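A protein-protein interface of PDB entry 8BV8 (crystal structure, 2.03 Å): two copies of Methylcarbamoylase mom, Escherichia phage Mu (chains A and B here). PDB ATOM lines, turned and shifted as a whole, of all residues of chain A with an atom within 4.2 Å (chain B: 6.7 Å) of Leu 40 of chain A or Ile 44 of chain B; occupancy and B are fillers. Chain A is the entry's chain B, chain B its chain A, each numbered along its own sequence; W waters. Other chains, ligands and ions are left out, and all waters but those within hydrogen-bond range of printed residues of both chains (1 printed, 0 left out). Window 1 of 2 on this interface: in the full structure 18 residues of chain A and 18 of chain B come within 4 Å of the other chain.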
ATOM      1  N   SER A  37     -30.745 -33.221 -17.416  1.00  0.00           N
ATOM      2  CA  SER A  37     -31.918 -32.534 -16.903  1.00  0.00           C
ATOM      3  C   SER A  37     -32.038 -31.140 -17.512  1.00  0.00           C
ATOM      4  O   SER A  37     -31.067 -30.554 -17.997  1.00  0.00           O
ATOM      5  CB  SER A  37     -31.861 -32.433 -15.377  1.00  0.00           C
ATOM      6  OG  SER A  37     -30.897 -31.481 -14.962  1.00  0.00           O
ATOM      7  N   CYS A  38     -33.263 -30.609 -17.478  1.00  0.00           N
ATOM      8  CA  CYS A  38     -33.512 -29.295 -18.060  1.00  0.00           C
ATOM      9  C   CYS A  38     -32.803 -28.195 -17.279  1.00  0.00           C
ATOM     10  O   CYS A  38     -32.233 -27.274 -17.875  1.00  0.00           O
ATOM     11  CB  CYS A  38     -35.015 -29.025 -18.120  1.00  0.00           C
ATOM     12  SG  CYS A  38     -35.445 -27.379 -18.738  1.00  0.00           S
ATOM     13  N   TRP A  39     -32.825 -28.272 -15.943  1.00  0.00           N
ATOM     14  CA  TRP A  39     -32.186 -27.231 -15.145  1.00  0.00           C
ATOM     15  C   TRP A  39     -30.677 -27.210 -15.357  1.00  0.00           C
ATOM     16  O   TRP A  39     -30.067 -26.136 -15.336  1.00  0.00           O
ATOM     17  CB  TRP A  39     -32.515 -27.411 -13.657  1.00  0.00           C
ATOM     18  CG  TRP A  39     -31.850 -28.593 -13.000  1.00  0.00           C
ATOM     19  CD1 TRP A  39     -32.392 -29.831 -12.793  1.00  0.00           C
ATOM     20  CD2 TRP A  39     -30.527 -28.639 -12.451  1.00  0.00           C
ATOM     21  NE1 TRP A  39     -31.484 -30.644 -12.155  1.00  0.00           N
ATOM     22  CE2 TRP A  39     -30.332 -29.936 -11.935  1.00  0.00           C
ATOM     23  CE3 TRP A  39     -29.486 -27.709 -12.348  1.00  0.00           C
ATOM     24  CZ2 TRP A  39     -29.140 -30.326 -11.327  1.00  0.00           C
ATOM     25  CZ3 TRP A  39     -28.305 -28.099 -11.746  1.00  0.00           C
ATOM     26  CH2 TRP A  39     -28.141 -29.395 -11.244  1.00  0.00           C
ATOM     27  N   LEU A  40     -30.060 -28.374 -15.565  1.00  0.00           N
ATOM     28  CA  LEU A  40     -28.615 -28.409 -15.774  1.00  0.00           C
ATOM     29  C   LEU A  40     -28.243 -27.859 -17.145  1.00  0.00           C
ATOM     30  O   LEU A  40     -27.251 -27.132 -17.281  1.00  0.00           O
ATOM     31  CB  LEU A  40     -28.093 -29.836 -15.611  1.00  0.00           C
ATOM     32  CG  LEU A  40     -26.584 -30.015 -15.794  1.00  0.00           C
ATOM     33  CD1 LEU A  40     -25.812 -29.199 -14.768  1.00  0.00           C
ATOM     34  CD2 LEU A  40     -26.197 -31.483 -15.716  1.00  0.00           C
ATOM     35  N   ALA A  41     -29.030 -28.191 -18.170  1.00  0.00           N
ATOM     36  CA  ALA A  41     -28.764 -27.662 -19.503  1.00  0.00           C
ATOM     37  C   ALA A  41     -28.942 -26.150 -19.536  1.00  0.00           C
ATOM     38  O   ALA A  41     -28.113 -25.432 -20.107  1.00  0.00           O
ATOM     39  CB  ALA A  41     -29.678 -28.333 -20.530  1.00  0.00           C
ATOM     40  N   ARG A  42     -30.014 -25.647 -18.918  1.00  0.00           N
ATOM     41  CA  ARG A  42     -30.244 -24.206 -18.887  1.00  0.00           C
ATOM     42  C   ARG A  42     -29.160 -23.487 -18.097  1.00  0.00           C
ATOM     43  O   ARG A  42     -28.731 -22.390 -18.475  1.00  0.00           O
ATOM     44  CB  ARG A  42     -31.616 -23.903 -18.289  1.00  0.00           C
ATOM     45  CG  ARG A  42     -32.797 -24.286 -19.159  1.00  0.00           C
ATOM     46  CD  ARG A  42     -34.092 -23.925 -18.454  1.00  0.00           C
ATOM     47  NE  ARG A  42     -35.252 -23.995 -19.332  1.00  0.00           N
ATOM     48  CZ  ARG A  42     -36.476 -23.630 -18.977  1.00  0.00           C
ATOM     49  NH1 ARG A  42     -36.734 -23.164 -17.766  1.00  0.00           N
ATOM     50  NH2 ARG A  42     -37.466 -23.734 -19.860  1.00  0.00           N
ATOM     51  N   THR A  43     -28.713 -24.085 -16.989  1.00  0.00           N
ATOM     52  CA  THR A  43     -27.698 -23.450 -16.153  1.00  0.00           C
ATOM     53  C   THR A  43     -26.392 -23.274 -16.915  1.00  0.00           C
ATOM     54  O   THR A  43     -25.786 -22.195 -16.895  1.00  0.00           O
ATOM     55  CB  THR A  43     -27.476 -24.276 -14.883  1.00  0.00           C
ATOM     56  OG1 THR A  43     -28.665 -24.255 -14.083  1.00  0.00           O
ATOM     57  CG2 THR A  43     -26.318 -23.718 -14.074  1.00  0.00           C
ATOM     58  N   ILE A  44     -25.942 -24.328 -17.597  1.00  0.00           N
ATOM     59  CA  ILE A  44     -24.682 -24.261 -18.330  1.00  0.00           C
ATOM     60  C   ILE A  44     -24.794 -23.302 -19.508  1.00  0.00           C
ATOM     61  O   ILE A  44     -23.875 -22.519 -19.777  1.00  0.00           O
ATOM     62  CB  ILE A  44     -24.260 -25.670 -18.781  1.00  0.00           C
ATOM     63  CG1 ILE A  44     -23.966 -26.547 -17.563  1.00  0.00           C
ATOM     64  CG2 ILE A  44     -23.055 -25.602 -19.714  1.00  0.00           C
ATOM     65  CD1 ILE A  44     -23.699 -27.989 -17.901  1.00  0.00           C
ATOM     66  N   ILE B  36     -15.715 -33.537 -10.086  1.00  0.00           N
ATOM     67  CA  ILE B  36     -16.129 -32.926 -11.338  1.00  0.00           C
ATOM     68  C   ILE B  36     -15.160 -31.792 -11.650  1.00  0.00           C
ATOM     69  O   ILE B  36     -14.346 -31.394 -10.816  1.00  0.00           O
ATOM     70  CB  ILE B  36     -17.581 -32.407 -11.296  1.00  0.00           C
ATOM     71  CG1 ILE B  36     -17.765 -31.422 -10.139  1.00  0.00           C
ATOM     72  CG2 ILE B  36     -18.560 -33.568 -11.182  1.00  0.00           C
ATOM     73  CD1 ILE B  36     -19.158 -30.837 -10.053  1.00  0.00           C
ATOM     74  N   TRP B  39     -14.760 -25.819 -13.643  1.00  0.00           N
ATOM     75  CA  TRP B  39     -15.659 -24.903 -14.339  1.00  0.00           C
ATOM     76  C   TRP B  39     -17.118 -25.298 -14.135  1.00  0.00           C
ATOM     77  O   TRP B  39     -17.987 -24.432 -13.987  1.00  0.00           O
ATOM     78  CB  TRP B  39     -15.313 -24.847 -15.834  1.00  0.00           C
ATOM     79  CG  TRP B  39     -15.745 -26.056 -16.626  1.00  0.00           C
ATOM     80  CD1 TRP B  39     -14.975 -27.127 -16.978  1.00  0.00           C
ATOM     81  CD2 TRP B  39     -17.049 -26.306 -17.168  1.00  0.00           C
ATOM     82  NE1 TRP B  39     -15.721 -28.030 -17.697  1.00  0.00           N
ATOM     83  CE2 TRP B  39     -16.998 -27.550 -17.825  1.00  0.00           C
ATOM     84  CE3 TRP B  39     -18.258 -25.601 -17.152  1.00  0.00           C
ATOM     85  CZ2 TRP B  39     -18.107 -28.102 -18.464  1.00  0.00           C
ATOM     86  CZ3 TRP B  39     -19.356 -26.150 -17.783  1.00  0.00           C
ATOM     87  CH2 TRP B  39     -19.275 -27.388 -18.431  1.00  0.00           C
ATOM     88  N   LEU B  40     -17.405 -26.603 -14.114  1.00  0.00           N
ATOM     89  CA  LEU B  40     -18.787 -27.050 -13.968  1.00  0.00           C
ATOM     90  C   LEU B  40     -19.311 -26.784 -12.563  1.00  0.00           C
ATOM     91  O   LEU B  40     -20.457 -26.351 -12.394  1.00  0.00           O
ATOM     92  CB  LEU B  40     -18.897 -28.536 -14.307  1.00  0.00           C
ATOM     93  CG  LEU B  40     -20.280 -29.155 -14.090  1.00  0.00           C
ATOM     94  CD1 LEU B  40     -21.325 -28.450 -14.943  1.00  0.00           C
ATOM     95  CD2 LEU B  40     -20.262 -30.649 -14.379  1.00  0.00           C
ATOM     96  N   ALA B  41     -18.488 -27.036 -11.543  1.00  0.00           N
ATOM     97  CA  ALA B  41     -18.910 -26.768 -10.172  1.00  0.00           C
ATOM     98  C   ALA B  41     -19.165 -25.281  -9.958  1.00  0.00           C
ATOM     99  O   ALA B  41     -20.164 -24.897  -9.339  1.00  0.00           O
ATOM    100  CB  ALA B  41     -17.859 -27.284  -9.189  1.00  0.00           C
ATOM    101  N   ARG B  42     -18.273 -24.429 -10.471  1.00  0.00           N
ATOM    102  CA  ARG B  42     -18.468 -22.988 -10.345  1.00  0.00           C
ATOM    103  C   ARG B  42     -19.738 -22.536 -11.055  1.00  0.00           C
ATOM    104  O   ARG B  42     -20.455 -21.659 -10.558  1.00  0.00           O
ATOM    105  CB  ARG B  42     -17.259 -22.244 -10.910  1.00  0.00           C
ATOM    106  CG  ARG B  42     -16.007 -22.332 -10.064  1.00  0.00           C
ATOM    107  CD  ARG B  42     -14.877 -21.558 -10.723  1.00  0.00           C
ATOM    108  NE  ARG B  42     -13.701 -21.441  -9.869  1.00  0.00           N
ATOM    109  CZ  ARG B  42     -12.592 -20.800 -10.211  1.00  0.00           C
ATOM    110  NH1 ARG B  42     -12.473 -20.206 -11.388  1.00  0.00           N
ATOM    111  NH2 ARG B  42     -11.577 -20.754  -9.352  1.00  0.00           N
ATOM    112  N   THR B  43     -20.027 -23.117 -12.219  1.00  0.00           N
ATOM    113  CA  THR B  43     -21.195 -22.703 -12.991  1.00  0.00           C
ATOM    114  C   THR B  43     -22.487 -22.998 -12.237  1.00  0.00           C
ATOM    115  O   THR B  43     -23.372 -22.140 -12.142  1.00  0.00           O
ATOM    116  CB  THR B  43     -21.192 -23.398 -14.355  1.00  0.00           C
ATOM    117  OG1 THR B  43     -20.088 -22.920 -15.135  1.00  0.00           O
ATOM    118  CG2 THR B  43     -22.495 -23.129 -15.096  1.00  0.00           C
ATOM    119  N   ILE B  44     -22.609 -24.210 -11.690  1.00  0.00           N
ATOM    120  CA  ILE B  44     -23.816 -24.576 -10.954  1.00  0.00           C
ATOM    121  C   ILE B  44     -23.953 -23.733  -9.693  1.00  0.00           C
ATOM    122  O   ILE B  44     -25.047 -23.261  -9.361  1.00  0.00           O
ATOM    123  CB  ILE B  44     -23.805 -26.082 -10.632  1.00  0.00           C
ATOM    124  CG1 ILE B  44     -23.875 -26.900 -11.921  1.00  0.00           C
ATOM    125  CG2 ILE B  44     -24.958 -26.444  -9.698  1.00  0.00           C
ATOM    126  CD1 ILE B  44     -23.393 -28.320 -11.769  1.00  0.00           C
ATOM    127  N   ILE B  45     -22.847 -23.523  -8.977  1.00  0.00           N
ATOM    128  CA  ILE B  45     -22.908 -22.835  -7.690  1.00  0.00           C
ATOM    129  C   ILE B  45     -23.323 -21.379  -7.874  1.00  0.00           C
ATOM    130  O   ILE B  45     -24.244 -20.892  -7.210  1.00  0.00           O
ATOM    131  CB  ILE B  45     -21.561 -22.952  -6.953  1.00  0.00           C
ATOM    132  CG1 ILE B  45     -21.385 -24.361  -6.388  1.00  0.00           C
ATOM    133  CG2 ILE B  45     -21.468 -21.924  -5.832  1.00  0.00           C
ATOM    134  CD1 ILE B  45     -22.407 -24.724  -5.330  1.00  0.00           C
ATOM    135  N   GLN B  46     -22.660 -20.662  -8.787  1.00  0.00           N
ATOM    136  CA  GLN B  46     -22.972 -19.249  -8.973  1.00  0.00           C
ATOM    137  C   GLN B  46     -24.387 -19.031  -9.498  1.00  0.00           C
ATOM    138  O   GLN B  46     -24.909 -17.917  -9.389  1.00  0.00           O
ATOM    139  CB  GLN B  46     -21.961 -18.596  -9.918  1.00  0.00           C
ATOM    140  CG  GLN B  46     -22.240 -18.820 -11.393  1.00  0.00           C
ATOM    141  CD  GLN B  46     -21.286 -18.049 -12.286  1.00  0.00           C
ATOM    142  OE1 GLN B  46     -20.158 -17.750 -11.894  1.00  0.00           O
ATOM    143  NE2 GLN B  46     -21.740 -17.715 -13.487  1.00  0.00           N
ATOM    144  N   THR B  47     -25.019 -20.064 -10.048  1.00  0.00           N
ATOM    145  CA  THR B  47     -26.392 -19.965 -10.526  1.00  0.00           C
ATOM    146  C   THR B  47     -27.407 -20.366  -9.459  1.00  0.00           C
ATOM    147  O   THR B  47     -28.469 -19.742  -9.350  1.00  0.00           O
ATOM    148  CB  THR B  47     -26.576 -20.836 -11.773  1.00  0.00           C
ATOM    149  OG1 THR B  47     -25.721 -20.362 -12.821  1.00  0.00           O
ATOM    150  CG2 THR B  47     -28.022 -20.806 -12.251  1.00  0.00           C
ATOM    151  N   LYS B  48     -27.095 -21.383  -8.654  1.00  0.00           N
ATOM    152  CA  LYS B  48     -28.061 -21.973  -7.737  1.00  0.00           C
ATOM    153  C   LYS B  48     -27.847 -21.609  -6.274  1.00  0.00           C
ATOM    154  O   LYS B  48     -28.827 -21.493  -5.537  1.00  0.00           O
ATOM    155  CB  LYS B  48     -28.048 -23.501  -7.866  1.00  0.00           C
ATOM    156  CG  LYS B  48     -28.432 -24.013  -9.246  1.00  0.00           C
ATOM    157  CD  LYS B  48     -29.822 -23.542  -9.643  1.00  0.00           C
ATOM    158  CE  LYS B  48     -30.269 -24.174 -10.950  1.00  0.00           C
ATOM    159  NZ  LYS B  48     -31.587 -23.647 -11.401  1.00  0.00           N
ATOM    160  N   HIS B  49     -26.604 -21.441  -5.832  1.00  0.00           N
ATOM    161  CA  HIS B  49     -26.345 -21.140  -4.430  1.00  0.00           C
ATOM    162  C   HIS B  49     -26.912 -19.772  -4.063  1.00  0.00           C
ATOM    163  O   HIS B  49     -26.960 -18.854  -4.886  1.00  0.00           O
ATOM    164  CB  HIS B  49     -24.845 -21.186  -4.143  1.00  0.00           C
ATOM    165  CG  HIS B  49     -24.507 -21.217  -2.685  1.00  0.00           C
ATOM    166  ND1 HIS B  49     -24.200 -20.081  -1.966  1.00  0.00           N
ATOM    167  CD2 HIS B  49     -24.423 -22.249  -1.811  1.00  0.00           C
ATOM    168  CE1 HIS B  49     -23.942 -20.412  -0.714  1.00  0.00           C
ATOM    169  NE2 HIS B  49     -24.070 -21.721  -0.593  1.00  0.00           N
ATOM    170  N   LEU B  70     -26.781 -35.739 -12.140  1.00  0.00           N
ATOM    171  CA  LEU B  70     -26.079 -34.797 -11.276  1.00  0.00           C
ATOM    172  C   LEU B  70     -27.109 -33.928 -10.564  1.00  0.00           C
ATOM    173  O   LEU B  70     -27.936 -33.284 -11.217  1.00  0.00           O
ATOM    174  CB  LEU B  70     -25.119 -33.943 -12.102  1.00  0.00           C
ATOM    175  CG  LEU B  70     -24.433 -32.756 -11.427  1.00  0.00           C
ATOM    176  CD1 LEU B  70     -23.493 -33.225 -10.332  1.00  0.00           C
ATOM    177  CD2 LEU B  70     -23.686 -31.927 -12.461  1.00  0.00           C
ATOM    178  N   GLY B  72     -26.285 -32.102  -7.401  1.00  0.00           N
ATOM    179  CA  GLY B  72     -25.722 -31.215  -6.398  1.00  0.00           C
ATOM    180  C   GLY B  72     -24.236 -31.021  -6.592  1.00  0.00           C
ATOM    181  O   GLY B  72     -23.590 -31.708  -7.391  1.00  0.00           O
ATOM    182  N   VAL B  73     -23.699 -30.064  -5.833  1.00  0.00           N
ATOM    183  CA  VAL B  73     -22.285 -29.705  -5.878  1.00  0.00           C
ATOM    184  C   VAL B  73     -21.800 -29.420  -4.461  1.00  0.00           C
ATOM    185  O   VAL B  73     -22.482 -28.745  -3.684  1.00  0.00           O
ATOM    186  CB  VAL B  73     -22.032 -28.482  -6.786  1.00  0.00           C
ATOM    187  CG1 VAL B  73     -20.584 -28.030  -6.681  1.00  0.00           C
ATOM    188  CG2 VAL B  73     -22.386 -28.795  -8.233  1.00  0.00           C
ATOM    189  N   TRP B 104     -24.737 -27.052  -2.537  1.00  0.00           N
ATOM    190  CA  TRP B 104     -26.079 -26.906  -3.082  1.00  0.00           C
ATOM    191  C   TRP B 104     -26.555 -28.265  -3.564  1.00  0.00           C
ATOM    192  O   TRP B 104     -25.810 -28.981  -4.239  1.00  0.00           O
ATOM    193  CB  TRP B 104     -26.123 -25.894  -4.233  1.00  0.00           C
ATOM    194  CG  TRP B 104     -27.449 -25.882  -4.945  1.00  0.00           C
ATOM    195  CD1 TRP B 104     -28.555 -25.157  -4.608  1.00  0.00           C
ATOM    196  CD2 TRP B 104     -27.810 -26.649  -6.103  1.00  0.00           C
ATOM    197  NE1 TRP B 104     -29.580 -25.420  -5.485  1.00  0.00           N
ATOM    198  CE2 TRP B 104     -29.149 -26.334  -6.411  1.00  0.00           C
ATOM    199  CE3 TRP B 104     -27.131 -27.570  -6.907  1.00  0.00           C
ATOM    200  CZ2 TRP B 104     -29.819 -26.902  -7.494  1.00  0.00           C
ATOM    201  CZ3 TRP B 104     -27.800 -28.136  -7.980  1.00  0.00           C
ATOM    202  CH2 TRP B 104     -29.130 -27.799  -8.264  1.00  0.00           C
HETATM  203  O   HOH W   1     -29.398 -33.278 -13.361  1.00  0.00           O
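Along chain A the printed residues that touch a printed residue of chain B span positions 39 to 44. Printed residues of chain B that touch a printed residue of chain A: Leu 40, Thr 43, Ile 44, Thr 47, Lys 48, Leu 70 and Trp 104.
Trp 39 of chain A touches Lys 48 of chain B (CE3 to CE, 3.9 Å). Leu 70 of chain B touches Trp 39 of chain A. CH2 of Trp 39 of chain A touches CZ3 of Trp 104 of chain B, 3.5 Å away. CD1 of Ile 44 of chain B touches CD1 of Leu 40 of chain A (3.95 Å). O of Thr 43 of chain B touches CG2 of Thr 43 of chain A, 3.9 Å away. Thr 47 of chain B touches Thr 43 of chain A (OG1 to CG2, 3.6 Å). Thr 43 of chain A touches Lys 48 of chain B. Leu 40 of chain B touches Ile 44 of chain A.
Leu 40 of chain A touches Ile 44 of chain B, and with the chains exchanged Ile 44 of chain A touches Leu 40 of chain B. Thr 43 of chain A touches its own counterpart, Thr 43 of chain B.
Of chain B, only Ile 44 (3.95 Å) comes within 4 Å of Leu 40 of chain A. Of chain A, only Leu 40 comes within 4 Å of Ile 44 of chain B. Printed residues of chain A within 4 Å of Thr 43 of chain B: Thr 43 (3.9 Å). Of the printed residues of chain B, Trp 39 of chain A touches Lys 48, Leu 70 and Trp 104.
The backbone carbonyl oxygen (O) of Trp 39 of chain B is in hydrogen-bond range of the side-chain hydroxyl (OG1) of Thr 43 of chain B, 2.8 Å away. The backbone carbonyl oxygen (O) of Thr 43 of chain B sits at hydrogen-bond distance from the side-chain hydroxyl (OG1) of Thr 47 of chain B. The backbone NH (N) of Val 73 of chain B is in hydrogen-bond range of the backbone carbonyl oxygen (O) of Trp 104 of chain B (2.9 Å). The side-chain hydroxyl of Ser 37 of chain A lies within hydrogen-bond range of the indole nitrogen of Trp 39 of chain A, 3.0 Å away. OG of Ser 37 of chain A lies within hydrogen-bond range of N of Leu 40 of chain A. The backbone carbonyl oxygen (O) of Trp 39 of chain A is in hydrogen-bond range of the side-chain hydroxyl (OG1) of Thr 43 of chain A (2.7 Å).
Water W1 lies within hydrogen-bond range of O of Leu 70 of chain B (2.6 Å) and OG of Ser 37 of chain A (2.8 Å).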
